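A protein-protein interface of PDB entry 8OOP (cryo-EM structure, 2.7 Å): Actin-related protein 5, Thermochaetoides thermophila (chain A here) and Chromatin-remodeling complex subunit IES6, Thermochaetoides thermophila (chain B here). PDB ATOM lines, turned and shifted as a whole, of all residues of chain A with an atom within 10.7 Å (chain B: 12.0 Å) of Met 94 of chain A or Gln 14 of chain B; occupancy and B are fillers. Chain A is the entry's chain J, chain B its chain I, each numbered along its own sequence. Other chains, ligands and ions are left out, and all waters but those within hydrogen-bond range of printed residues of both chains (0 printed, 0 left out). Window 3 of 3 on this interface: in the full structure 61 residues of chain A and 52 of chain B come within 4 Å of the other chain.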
ATOM      1  N   TYR A  89       1.831 -17.021 -32.712  1.00  0.00           N
ATOM      2  CA  TYR A  89       2.006 -18.447 -32.454  1.00  0.00           C
ATOM      3  C   TYR A  89       1.191 -18.869 -31.237  1.00  0.00           C
ATOM      4  O   TYR A  89       0.747 -18.038 -30.441  1.00  0.00           O
ATOM      5  CB  TYR A  89       3.486 -18.800 -32.263  1.00  0.00           C
ATOM      6  CG  TYR A  89       4.136 -18.138 -31.069  1.00  0.00           C
ATOM      7  CD1 TYR A  89       4.120 -18.737 -29.816  1.00  0.00           C
ATOM      8  CD2 TYR A  89       4.777 -16.915 -31.196  1.00  0.00           C
ATOM      9  CE1 TYR A  89       4.707 -18.124 -28.722  1.00  0.00           C
ATOM     10  CE2 TYR A  89       5.375 -16.301 -30.111  1.00  0.00           C
ATOM     11  CZ  TYR A  89       5.334 -16.909 -28.876  1.00  0.00           C
ATOM     12  OH  TYR A  89       5.938 -16.304 -27.797  1.00  0.00           O
ATOM     13  N   ARG A  90       1.009 -20.185 -31.109  1.00  0.00           N
ATOM     14  CA  ARG A  90       0.429 -20.817 -29.927  1.00  0.00           C
ATOM     15  C   ARG A  90       1.549 -21.327 -29.025  1.00  0.00           C
ATOM     16  O   ARG A  90       2.388 -22.121 -29.464  1.00  0.00           O
ATOM     17  CB  ARG A  90      -0.488 -21.971 -30.336  1.00  0.00           C
ATOM     18  CG  ARG A  90      -1.511 -22.395 -29.290  1.00  0.00           C
ATOM     19  CD  ARG A  90      -2.749 -21.511 -29.329  1.00  0.00           C
ATOM     20  NE  ARG A  90      -3.699 -21.842 -28.274  1.00  0.00           N
ATOM     21  CZ  ARG A  90      -4.937 -21.367 -28.206  1.00  0.00           C
ATOM     22  NH1 ARG A  90      -5.379 -20.461 -29.062  1.00  0.00           N
ATOM     23  NH2 ARG A  90      -5.742 -21.794 -27.237  1.00  0.00           N
ATOM     24  N   ASP A  91       1.562 -20.875 -27.772  1.00  0.00           N
ATOM     25  CA  ASP A  91       2.564 -21.333 -26.814  1.00  0.00           C
ATOM     26  C   ASP A  91       2.306 -22.797 -26.464  1.00  0.00           C
ATOM     27  O   ASP A  91       1.265 -23.132 -25.891  1.00  0.00           O
ATOM     28  CB  ASP A  91       2.530 -20.450 -25.565  1.00  0.00           C
ATOM     29  CG  ASP A  91       3.577 -20.838 -24.517  1.00  0.00           C
ATOM     30  OD1 ASP A  91       3.885 -22.035 -24.338  1.00  0.00           O
ATOM     31  OD2 ASP A  91       4.107 -19.916 -23.862  1.00  0.00           O
ATOM     32  N   ARG A  92       3.259 -23.666 -26.813  1.00  0.00           N
ATOM     33  CA  ARG A  92       3.087 -25.104 -26.624  1.00  0.00           C
ATOM     34  C   ARG A  92       3.008 -25.506 -25.155  1.00  0.00           C
ATOM     35  O   ARG A  92       2.478 -26.580 -24.851  1.00  0.00           O
ATOM     36  CB  ARG A  92       4.215 -25.862 -27.330  1.00  0.00           C
ATOM     37  CG  ARG A  92       4.249 -25.590 -28.827  1.00  0.00           C
ATOM     38  CD  ARG A  92       5.213 -26.489 -29.582  1.00  0.00           C
ATOM     39  NE  ARG A  92       5.298 -26.092 -30.983  1.00  0.00           N
ATOM     40  CZ  ARG A  92       5.614 -26.904 -31.983  1.00  0.00           C
ATOM     41  NH1 ARG A  92       5.901 -28.178 -31.776  1.00  0.00           N
ATOM     42  NH2 ARG A  92       5.646 -26.424 -33.224  1.00  0.00           N
ATOM     43  N   LYS A  93       3.514 -24.679 -24.242  1.00  0.00           N
ATOM     44  CA  LYS A  93       3.413 -24.966 -22.816  1.00  0.00           C
ATOM     45  C   LYS A  93       2.188 -24.310 -22.183  1.00  0.00           C
ATOM     46  O   LYS A  93       1.440 -24.966 -21.453  1.00  0.00           O
ATOM     47  CB  LYS A  93       4.689 -24.512 -22.096  1.00  0.00           C
ATOM     48  CG  LYS A  93       5.961 -25.186 -22.593  1.00  0.00           C
ATOM     49  CD  LYS A  93       7.175 -24.758 -21.779  1.00  0.00           C
ATOM     50  CE  LYS A  93       8.451 -25.388 -22.320  1.00  0.00           C
ATOM     51  NZ  LYS A  93       9.642 -25.042 -21.497  1.00  0.00           N
ATOM     52  N   MET A  94       1.974 -23.021 -22.451  1.00  0.00           N
ATOM     53  CA  MET A  94       0.890 -22.283 -21.812  1.00  0.00           C
ATOM     54  C   MET A  94      -0.456 -22.497 -22.500  1.00  0.00           C
ATOM     55  O   MET A  94      -1.500 -22.321 -21.860  1.00  0.00           O
ATOM     56  CB  MET A  94       1.234 -20.791 -21.766  1.00  0.00           C
ATOM     57  CG  MET A  94       0.273 -19.943 -20.948  1.00  0.00           C
ATOM     58  SD  MET A  94       0.825 -18.237 -20.763  1.00  0.00           S
ATOM     59  CE  MET A  94       2.147 -18.437 -19.573  1.00  0.00           C
ATOM     60  N   GLY A  95      -0.458 -22.885 -23.775  1.00  0.00           N
ATOM     61  CA  GLY A  95      -1.673 -23.271 -24.468  1.00  0.00           C
ATOM     62  C   GLY A  95      -2.524 -22.145 -25.016  1.00  0.00           C
ATOM     63  O   GLY A  95      -3.673 -22.395 -25.400  1.00  0.00           O
ATOM     64  N   LYS A  96      -2.009 -20.919 -25.065  1.00  0.00           N
ATOM     65  CA  LYS A  96      -2.746 -19.768 -25.565  1.00  0.00           C
ATOM     66  C   LYS A  96      -2.010 -19.161 -26.756  1.00  0.00           C
ATOM     67  O   LYS A  96      -0.796 -19.324 -26.911  1.00  0.00           O
ATOM     68  CB  LYS A  96      -2.961 -18.721 -24.467  1.00  0.00           C
ATOM     69  CG  LYS A  96      -1.721 -17.955 -24.084  1.00  0.00           C
ATOM     70  CD  LYS A  96      -2.055 -16.805 -23.154  1.00  0.00           C
ATOM     71  CE  LYS A  96      -2.562 -17.309 -21.816  1.00  0.00           C
ATOM     72  NZ  LYS A  96      -2.851 -16.184 -20.887  1.00  0.00           N
ATOM     73  N   THR A  97      -2.762 -18.457 -27.602  1.00  0.00           N
ATOM     74  CA  THR A  97      -2.176 -17.689 -28.696  1.00  0.00           C
ATOM     75  C   THR A  97      -1.518 -16.406 -28.195  1.00  0.00           C
ATOM     76  O   THR A  97      -2.039 -15.723 -27.310  1.00  0.00           O
ATOM     77  CB  THR A  97      -3.247 -17.355 -29.739  1.00  0.00           C
ATOM     78  OG1 THR A  97      -3.766 -18.569 -30.293  1.00  0.00           O
ATOM     79  CG2 THR A  97      -2.669 -16.513 -30.869  1.00  0.00           C
ATOM     80  N   PHE A  98      -0.360 -16.090 -28.776  1.00  0.00           N
ATOM     81  CA  PHE A  98       0.307 -14.803 -28.641  1.00  0.00           C
ATOM     82  C   PHE A  98       0.466 -14.156 -30.013  1.00  0.00           C
ATOM     83  O   PHE A  98       0.623 -14.847 -31.022  1.00  0.00           O
ATOM     84  CB  PHE A  98       1.683 -14.966 -27.986  1.00  0.00           C
ATOM     85  CG  PHE A  98       1.622 -15.312 -26.529  1.00  0.00           C
ATOM     86  CD1 PHE A  98       1.531 -16.632 -26.127  1.00  0.00           C
ATOM     87  CD2 PHE A  98       1.663 -14.324 -25.562  1.00  0.00           C
ATOM     88  CE1 PHE A  98       1.478 -16.962 -24.788  1.00  0.00           C
ATOM     89  CE2 PHE A  98       1.608 -14.647 -24.219  1.00  0.00           C
ATOM     90  CZ  PHE A  98       1.514 -15.970 -23.832  1.00  0.00           C
ATOM     91  N   SER A  99       0.420 -12.823 -30.049  1.00  0.00           N
ATOM     92  CA  SER A  99       0.605 -12.092 -31.298  1.00  0.00           C
ATOM     93  C   SER A  99       1.417 -10.825 -31.070  1.00  0.00           C
ATOM     94  O   SER A  99       1.266 -10.149 -30.050  1.00  0.00           O
ATOM     95  CB  SER A  99      -0.740 -11.733 -31.937  1.00  0.00           C
ATOM     96  OG  SER A  99      -0.554 -11.174 -33.225  1.00  0.00           O
ATOM     97  N   PHE A 100       2.285 -10.522 -32.038  1.00  0.00           N
ATOM     98  CA  PHE A 100       3.233  -9.417 -31.978  1.00  0.00           C
ATOM     99  C   PHE A 100       3.360  -8.816 -33.369  1.00  0.00           C
ATOM    100  O   PHE A 100       3.176  -9.514 -34.369  1.00  0.00           O
ATOM    101  CB  PHE A 100       4.601  -9.887 -31.478  1.00  0.00           C
ATOM    102  CG  PHE A 100       4.535 -10.657 -30.197  1.00  0.00           C
ATOM    103  CD1 PHE A 100       4.359 -10.011 -28.987  1.00  0.00           C
ATOM    104  CD2 PHE A 100       4.610 -12.039 -30.209  1.00  0.00           C
ATOM    105  CE1 PHE A 100       4.283 -10.730 -27.810  1.00  0.00           C
ATOM    106  CE2 PHE A 100       4.532 -12.761 -29.037  1.00  0.00           C
ATOM    107  CZ  PHE A 100       4.368 -12.106 -27.836  1.00  0.00           C
ATOM    108  N   TYR A 106      10.896 -10.315 -30.759  1.00  0.00           N
ATOM    109  CA  TYR A 106      12.248 -10.094 -30.254  1.00  0.00           C
ATOM    110  C   TYR A 106      13.250  -9.764 -31.350  1.00  0.00           C
ATOM    111  O   TYR A 106      14.340  -9.275 -31.039  1.00  0.00           O
ATOM    112  CB  TYR A 106      12.743 -11.315 -29.475  1.00  0.00           C
ATOM    113  CG  TYR A 106      12.226 -11.423 -28.062  1.00  0.00           C
ATOM    114  CD1 TYR A 106      11.075 -10.761 -27.661  1.00  0.00           C
ATOM    115  CD2 TYR A 106      12.913 -12.171 -27.116  1.00  0.00           C
ATOM    116  CE1 TYR A 106      10.613 -10.858 -26.364  1.00  0.00           C
ATOM    117  CE2 TYR A 106      12.462 -12.272 -25.818  1.00  0.00           C
ATOM    118  CZ  TYR A 106      11.311 -11.614 -25.445  1.00  0.00           C
ATOM    119  OH  TYR A 106      10.866 -11.713 -24.147  1.00  0.00           O
ATOM    120  N   ALA A 111      10.242 -14.087 -28.810  1.00  0.00           N
ATOM    121  CA  ALA A 111      11.095 -15.098 -28.199  1.00  0.00           C
ATOM    122  C   ALA A 111      11.132 -16.365 -29.048  1.00  0.00           C
ATOM    123  O   ALA A 111      11.940 -17.261 -28.808  1.00  0.00           O
ATOM    124  CB  ALA A 111      10.618 -15.414 -26.791  1.00  0.00           C
ATOM    125  N   ARG A 112      10.251 -16.427 -30.051  1.00  0.00           N
ATOM    126  CA  ARG A 112      10.133 -17.591 -30.919  1.00  0.00           C
ATOM    127  C   ARG A 112      10.301 -17.268 -32.399  1.00  0.00           C
ATOM    128  O   ARG A 112      10.551 -18.190 -33.185  1.00  0.00           O
ATOM    129  CB  ARG A 112       8.780 -18.290 -30.703  1.00  0.00           C
ATOM    130  CG  ARG A 112       8.510 -18.714 -29.256  1.00  0.00           C
ATOM    131  CD  ARG A 112       9.527 -19.731 -28.743  1.00  0.00           C
ATOM    132  NE  ARG A 112       9.349 -20.012 -27.322  1.00  0.00           N
ATOM    133  CZ  ARG A 112      10.168 -19.604 -26.360  1.00  0.00           C
ATOM    134  NH1 ARG A 112      11.210 -18.832 -26.619  1.00  0.00           N
ATOM    135  NH2 ARG A 112       9.922 -19.965 -25.102  1.00  0.00           N
ATOM    136  N   GLN B   7      10.684 -20.829 -11.642  1.00  0.00           N
ATOM    137  CA  GLN B   7      11.806 -19.920 -11.444  1.00  0.00           C
ATOM    138  C   GLN B   7      11.406 -18.504 -11.865  1.00  0.00           C
ATOM    139  O   GLN B   7      10.775 -18.306 -12.902  1.00  0.00           O
ATOM    140  CB  GLN B   7      13.039 -20.405 -12.211  1.00  0.00           C
ATOM    141  CG  GLN B   7      14.283 -19.562 -11.992  1.00  0.00           C
ATOM    142  CD  GLN B   7      15.515 -20.177 -12.623  1.00  0.00           C
ATOM    143  OE1 GLN B   7      15.425 -21.158 -13.362  1.00  0.00           O
ATOM    144  NE2 GLN B   7      16.680 -19.610 -12.326  1.00  0.00           N
ATOM    145  N   SER B   8      11.782 -17.533 -11.029  1.00  0.00           N
ATOM    146  CA  SER B   8      11.342 -16.150 -11.198  1.00  0.00           C
ATOM    147  C   SER B   8      11.700 -15.581 -12.569  1.00  0.00           C
ATOM    148  O   SER B   8      10.920 -14.816 -13.150  1.00  0.00           O
ATOM    149  CB  SER B   8      11.944 -15.281 -10.093  1.00  0.00           C
ATOM    150  OG  SER B   8      11.491 -13.942 -10.188  1.00  0.00           O
ATOM    151  N   ALA B   9      12.874 -15.931 -13.097  1.00  0.00           N
ATOM    152  CA  ALA B   9      13.265 -15.462 -14.426  1.00  0.00           C
ATOM    153  C   ALA B   9      12.290 -15.904 -15.514  1.00  0.00           C
ATOM    154  O   ALA B   9      11.934 -15.108 -16.393  1.00  0.00           O
ATOM    155  CB  ALA B   9      14.678 -15.947 -14.752  1.00  0.00           C
ATOM    156  N   GLN B  10      11.839 -17.158 -15.475  1.00  0.00           N
ATOM    157  CA  GLN B  10      10.862 -17.620 -16.459  1.00  0.00           C
ATOM    158  C   GLN B  10       9.496 -16.969 -16.257  1.00  0.00           C
ATOM    159  O   GLN B  10       8.810 -16.646 -17.234  1.00  0.00           O
ATOM    160  CB  GLN B  10      10.761 -19.148 -16.405  1.00  0.00           C
ATOM    161  CG  GLN B  10       9.855 -19.780 -17.460  1.00  0.00           C
ATOM    162  CD  GLN B  10       8.402 -19.870 -17.034  1.00  0.00           C
ATOM    163  OE1 GLN B  10       8.048 -19.523 -15.908  1.00  0.00           O
ATOM    164  NE2 GLN B  10       7.550 -20.342 -17.938  1.00  0.00           N
ATOM    165  N   ALA B  11       9.082 -16.769 -15.004  1.00  0.00           N
ATOM    166  CA  ALA B  11       7.833 -16.060 -14.736  1.00  0.00           C
ATOM    167  C   ALA B  11       7.876 -14.617 -15.231  1.00  0.00           C
ATOM    168  O   ALA B  11       6.920 -14.138 -15.853  1.00  0.00           O
ATOM    169  CB  ALA B  11       7.520 -16.101 -13.240  1.00  0.00           C
ATOM    170  N   ALA B  12       8.977 -13.912 -14.968  1.00  0.00           N
ATOM    171  CA  ALA B  12       9.149 -12.557 -15.485  1.00  0.00           C
ATOM    172  C   ALA B  12       9.187 -12.524 -17.010  1.00  0.00           C
ATOM    173  O   ALA B  12       8.637 -11.607 -17.632  1.00  0.00           O
ATOM    174  CB  ALA B  12      10.422 -11.936 -14.909  1.00  0.00           C
ATOM    175  N   HIS B  13       9.828 -13.516 -17.629  1.00  0.00           N
ATOM    176  CA  HIS B  13       9.826 -13.617 -19.086  1.00  0.00           C
ATOM    177  C   HIS B  13       8.410 -13.762 -19.641  1.00  0.00           C
ATOM    178  O   HIS B  13       8.019 -13.035 -20.560  1.00  0.00           O
ATOM    179  CB  HIS B  13      10.709 -14.790 -19.517  1.00  0.00           C
ATOM    180  CG  HIS B  13      10.805 -14.972 -20.999  1.00  0.00           C
ATOM    181  ND1 HIS B  13       9.808 -15.556 -21.749  1.00  0.00           N
ATOM    182  CD2 HIS B  13      11.792 -14.655 -21.871  1.00  0.00           C
ATOM    183  CE1 HIS B  13      10.172 -15.582 -23.019  1.00  0.00           C
ATOM    184  NE2 HIS B  13      11.373 -15.042 -23.119  1.00  0.00           N
ATOM    185  N   GLN B  14       7.626 -14.697 -19.098  1.00  0.00           N
ATOM    186  CA  GLN B  14       6.229 -14.823 -19.513  1.00  0.00           C
ATOM    187  C   GLN B  14       5.421 -13.564 -19.213  1.00  0.00           C
ATOM    188  O   GLN B  14       4.543 -13.183 -19.997  1.00  0.00           O
ATOM    189  CB  GLN B  14       5.585 -16.040 -18.848  1.00  0.00           C
ATOM    190  CG  GLN B  14       5.963 -17.373 -19.479  1.00  0.00           C
ATOM    191  CD  GLN B  14       5.317 -17.594 -20.840  1.00  0.00           C
ATOM    192  OE1 GLN B  14       4.687 -16.698 -21.403  1.00  0.00           O
ATOM    193  NE2 GLN B  14       5.475 -18.799 -21.376  1.00  0.00           N
ATOM    194  N   ALA B  15       5.696 -12.906 -18.084  1.00  0.00           N
ATOM    195  CA  ALA B  15       5.025 -11.644 -17.780  1.00  0.00           C
ATOM    196  C   ALA B  15       5.347 -10.567 -18.810  1.00  0.00           C
ATOM    197  O   ALA B  15       4.460  -9.813 -19.227  1.00  0.00           O
ATOM    198  CB  ALA B  15       5.409 -11.174 -16.378  1.00  0.00           C
ATOM    199  N   LEU B  16       6.607 -10.487 -19.239  1.00  0.00           N
ATOM    200  CA  LEU B  16       6.979  -9.558 -20.303  1.00  0.00           C
ATOM    201  C   LEU B  16       6.298  -9.907 -21.622  1.00  0.00           C
ATOM    202  O   LEU B  16       5.761  -9.030 -22.308  1.00  0.00           O
ATOM    203  CB  LEU B  16       8.499  -9.549 -20.462  1.00  0.00           C
ATOM    204  CG  LEU B  16       9.084  -8.752 -21.623  1.00  0.00           C
ATOM    205  CD1 LEU B  16       8.705  -7.286 -21.501  1.00  0.00           C
ATOM    206  CD2 LEU B  16      10.595  -8.916 -21.655  1.00  0.00           C
ATOM    207  N   VAL B  17       6.315 -11.187 -21.996  1.00  0.00           N
ATOM    208  CA  VAL B  17       5.650 -11.632 -23.221  1.00  0.00           C
ATOM    209  C   VAL B  17       4.148 -11.366 -23.168  1.00  0.00           C
ATOM    210  O   VAL B  17       3.538 -10.970 -24.170  1.00  0.00           O
ATOM    211  CB  VAL B  17       5.949 -13.123 -23.474  1.00  0.00           C
ATOM    212  CG1 VAL B  17       5.142 -13.643 -24.653  1.00  0.00           C
ATOM    213  CG2 VAL B  17       7.437 -13.333 -23.714  1.00  0.00           C
ATOM    214  N   GLU B  18       3.530 -11.562 -22.003  1.00  0.00           N
ATOM    215  CA  GLU B  18       2.130 -11.180 -21.827  1.00  0.00           C
ATOM    216  C   GLU B  18       1.920  -9.673 -21.942  1.00  0.00           C
ATOM    217  O   GLU B  18       0.927  -9.224 -22.526  1.00  0.00           O
ATOM    218  CB  GLU B  18       1.622 -11.679 -20.475  1.00  0.00           C
ATOM    219  CG  GLU B  18       1.329 -13.171 -20.426  1.00  0.00           C
ATOM    220  CD  GLU B  18      -0.049 -13.520 -20.955  1.00  0.00           C
ATOM    221  OE1 GLU B  18      -0.559 -12.796 -21.837  1.00  0.00           O
ATOM    222  OE2 GLU B  18      -0.626 -14.521 -20.483  1.00  0.00           O
ATOM    223  N   GLN B  19       2.841  -8.879 -21.396  1.00  0.00           N
ATOM    224  CA  GLN B  19       2.750  -7.427 -21.525  1.00  0.00           C
ATOM    225  C   GLN B  19       2.894  -6.973 -22.976  1.00  0.00           C
ATOM    226  O   GLN B  19       2.223  -6.028 -23.407  1.00  0.00           O
ATOM    227  CB  GLN B  19       3.806  -6.776 -20.632  1.00  0.00           C
ATOM    228  CG  GLN B  19       3.916  -5.270 -20.736  1.00  0.00           C
ATOM    229  CD  GLN B  19       4.879  -4.707 -19.708  1.00  0.00           C
ATOM    230  OE1 GLN B  19       5.345  -5.425 -18.822  1.00  0.00           O
ATOM    231  NE2 GLN B  19       5.173  -3.417 -19.810  1.00  0.00           N
ATOM    232  N   LEU B  20       3.764  -7.636 -23.741  1.00  0.00           N
ATOM    233  CA  LEU B  20       3.956  -7.341 -25.159  1.00  0.00           C
ATOM    234  C   LEU B  20       2.815  -7.825 -26.053  1.00  0.00           C
ATOM    235  O   LEU B  20       2.670  -7.316 -27.169  1.00  0.00           O
ATOM    236  CB  LEU B  20       5.270  -7.963 -25.624  1.00  0.00           C
ATOM    237  CG  LEU B  20       6.526  -7.301 -25.062  1.00  0.00           C
ATOM    238  CD1 LEU B  20       7.722  -8.225 -25.218  1.00  0.00           C
ATOM    239  CD2 LEU B  20       6.779  -5.958 -25.730  1.00  0.00           C
ATOM    240  N   ASP B  21       2.020  -8.792 -25.602  1.00  0.00           N
ATOM    241  CA  ASP B  21       1.035  -9.450 -26.459  1.00  0.00           C
ATOM    242  C   ASP B  21      -0.050  -8.508 -26.974  1.00  0.00           C
ATOM    243  O   ASP B  21      -0.652  -7.748 -26.211  1.00  0.00           O
ATOM    244  CB  ASP B  21       0.383 -10.605 -25.704  1.00  0.00           C
ATOM    245  CG  ASP B  21      -0.669 -11.310 -26.531  1.00  0.00           C
ATOM    246  OD1 ASP B  21      -0.421 -11.541 -27.733  1.00  0.00           O
ATOM    247  OD2 ASP B  21      -1.748 -11.621 -25.986  1.00  0.00           O
ATOM    248  N   LEU B  22      -0.282  -8.560 -28.293  1.00  0.00           N
ATOM    249  CA  LEU B  22      -1.421  -7.903 -28.928  1.00  0.00           C
ATOM    250  C   LEU B  22      -2.700  -8.731 -28.905  1.00  0.00           C
ATOM    251  O   LEU B  22      -3.788  -8.158 -29.022  1.00  0.00           O
ATOM    252  CB  LEU B  22      -1.103  -7.573 -30.383  1.00  0.00           C
ATOM    253  CG  LEU B  22       0.035  -6.605 -30.661  1.00  0.00           C
ATOM    254  CD1 LEU B  22       0.230  -6.531 -32.147  1.00  0.00           C
ATOM    255  CD2 LEU B  22      -0.297  -5.242 -30.090  1.00  0.00           C
ATOM    256  N   HIS B  23      -2.598 -10.056 -28.778  1.00  0.00           N
ATOM    257  CA  HIS B  23      -3.786 -10.902 -28.852  1.00  0.00           C
ATOM    258  C   HIS B  23      -4.730 -10.653 -27.683  1.00  0.00           C
ATOM    259  O   HIS B  23      -5.952 -10.752 -27.840  1.00  0.00           O
ATOM    260  CB  HIS B  23      -3.375 -12.376 -28.897  1.00  0.00           C
ATOM    261  CG  HIS B  23      -4.447 -13.291 -29.400  1.00  0.00           C
ATOM    262  ND1 HIS B  23      -4.870 -13.299 -30.711  1.00  0.00           N
ATOM    263  CD2 HIS B  23      -5.178 -14.240 -28.766  1.00  0.00           C
ATOM    264  CE1 HIS B  23      -5.819 -14.206 -30.862  1.00  0.00           C
ATOM    265  NE2 HIS B  23      -6.024 -14.792 -29.696  1.00  0.00           N
ATOM    266  N   SER B  24      -4.182 -10.317 -26.517  1.00  0.00           N
ATOM    267  CA  SER B  24      -4.948  -9.912 -25.345  1.00  0.00           C
ATOM    268  C   SER B  24      -5.686  -8.585 -25.505  1.00  0.00           C
ATOM    269  O   SER B  24      -6.474  -8.236 -24.619  1.00  0.00           O
ATOM    270  CB  SER B  24      -4.017  -9.825 -24.135  1.00  0.00           C
ATOM    271  OG  SER B  24      -3.397 -11.074 -23.879  1.00  0.00           O
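The side-chain carboxylate (OD2) of Asp 91 of chain A sits at hydrogen-bond distance from the side-chain amide nitrogen (NE2) of Gln 14 of chain B (3.0 Å). OE2 of Glu 18 of chain B is in salt-bridge range of NZ of Lys 96 of chain A, 2.8 Å away. The backbone NH (N) of Ser 99 of chain A lies within hydrogen-bond range of the side-chain carboxylate (OD1) of Asp 21 of chain B, at 2.8 Å. The backbone carbonyl oxygen (O) of Ser 99 of chain A is in hydrogen-bond range of the backbone NH (N) of Leu 22 of chain B, at 2.8 Å.
Asp 91 of chain A touches one residue of chain B. No residue of chain B comes within 4 Å of Lys 93 of chain A. Of the printed residues of chain B, Met 94 of chain A touches Gln 14 and Glu 18. No residue of chain B comes within 4 Å of Gly 95 of chain A. Printed residues of chain B within 4 Å of Thr 97 of chain A: His 23 (3.8 Å). Gln 7 of chain B touches none of the printed residues of chain A. No residue of chain A comes within 4 Å of Ala 12 of chain B. His 13 of chain B touches two residues of chain A. Printed residues of chain A within 4 Å of Gln 14 of chain B: Asp 91 and Met 94. No residue of chain A comes within 4 Å of Ala 15 of chain B. Of the printed residues of chain A, Leu 16 of chain B touches Tyr 106. Of chain A, only Phe 98 (3.7 Å), Phe 100 (3.6 Å) and Tyr 106 (3.8 Å) come within 4 Å of Val 17 of chain B. Printed residues of chain A within 4 Å of Glu 18 of chain B: Met 94, Lys 96 and Phe 98. Printed residues of chain A within 4 Å of Asp 21 of chain B: Phe 98 (3.5 Å), Ser 99 (2.8 Å) and Phe 100 (3.7 Å). Printed residues of chain A within 4 Å of Leu 22 of chain B: Ser 99. The nearest residue of chain A that does not touch Gln 14 of chain B is Phe 98 of chain A (4.1 Å).
The side-chain carboxylate (OD1) of Asp 21 of chain B is in hydrogen-bond range of the backbone NH (N) of His 23 of chain B, 2.8 Å away. The side-chain hydroxyl (OG) of Ser 24 of chain B sits at hydrogen-bond distance from the side-chain carboxylate (OD2) of Asp 21 of chain B, at 2.7 Å. The backbone carbonyl oxygen of Tyr 89 of chain A sits at hydrogen-bond distance from the backbone NH of Phe 98 of chain A (2.8 Å). The guanidinium group of Arg 90 of chain A is in hydrogen-bond range of the side-chain hydroxyl of Thr 97 of chain A (2.8 Å). The side-chain carboxylate of Asp 91 of chain A lies within hydrogen-bond range of the backbone NH of Lys 93 of chain A (2.7 Å). The backbone carbonyl oxygen (O) of Lys 96 of chain A sits at hydrogen-bond distance from the backbone NH (N) of Asp 91 of chain A, 3.0 Å away.
Of the 18 printed residues of chain B, 9 touch a printed residue of chain A. Among the printed residues, Asp or Glu carboxylates within 4 Å of a Lys or Arg side-chain nitrogen of the other chain: Lys 96 of chain A with Glu 18 of chain B.
Among the printed residues, pairs that only touch across the chains: Met 94 of chain A with Gln 14 of chain B (3.5 Å), Met 94 of chain A with Glu 18 of chain B (3.999 Å), Thr 97 of chain A with His 23 of chain B (3.8 Å), Phe 98 of chain A with Val 17 of chain B (3.7 Å), Phe 98 of chain A with Glu 18 of chain B (3.7 Å), Phe 98 of chain A with Asp 21 of chain B (3.5 Å), Ser 99 of chain A with His 23 of chain B (3.99 Å), Phe 100 of chain A with Val 17 of chain B (3.6 Å), Phe 100 of chain A with Leu 20 of chain B (3.7 Å), Phe 100 of chain A with Asp 21 of chain B (3.7 Å), Tyr 106 of chain A with His 13 of chain B (3.5 Å), Tyr 106 of chain A with Leu 16 of chain B (3.8 Å), Tyr 106 of chain A with Val 17 of chain B (3.8 Å) and Ala 111 of chain A with His 13 of chain B (3.8 Å).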
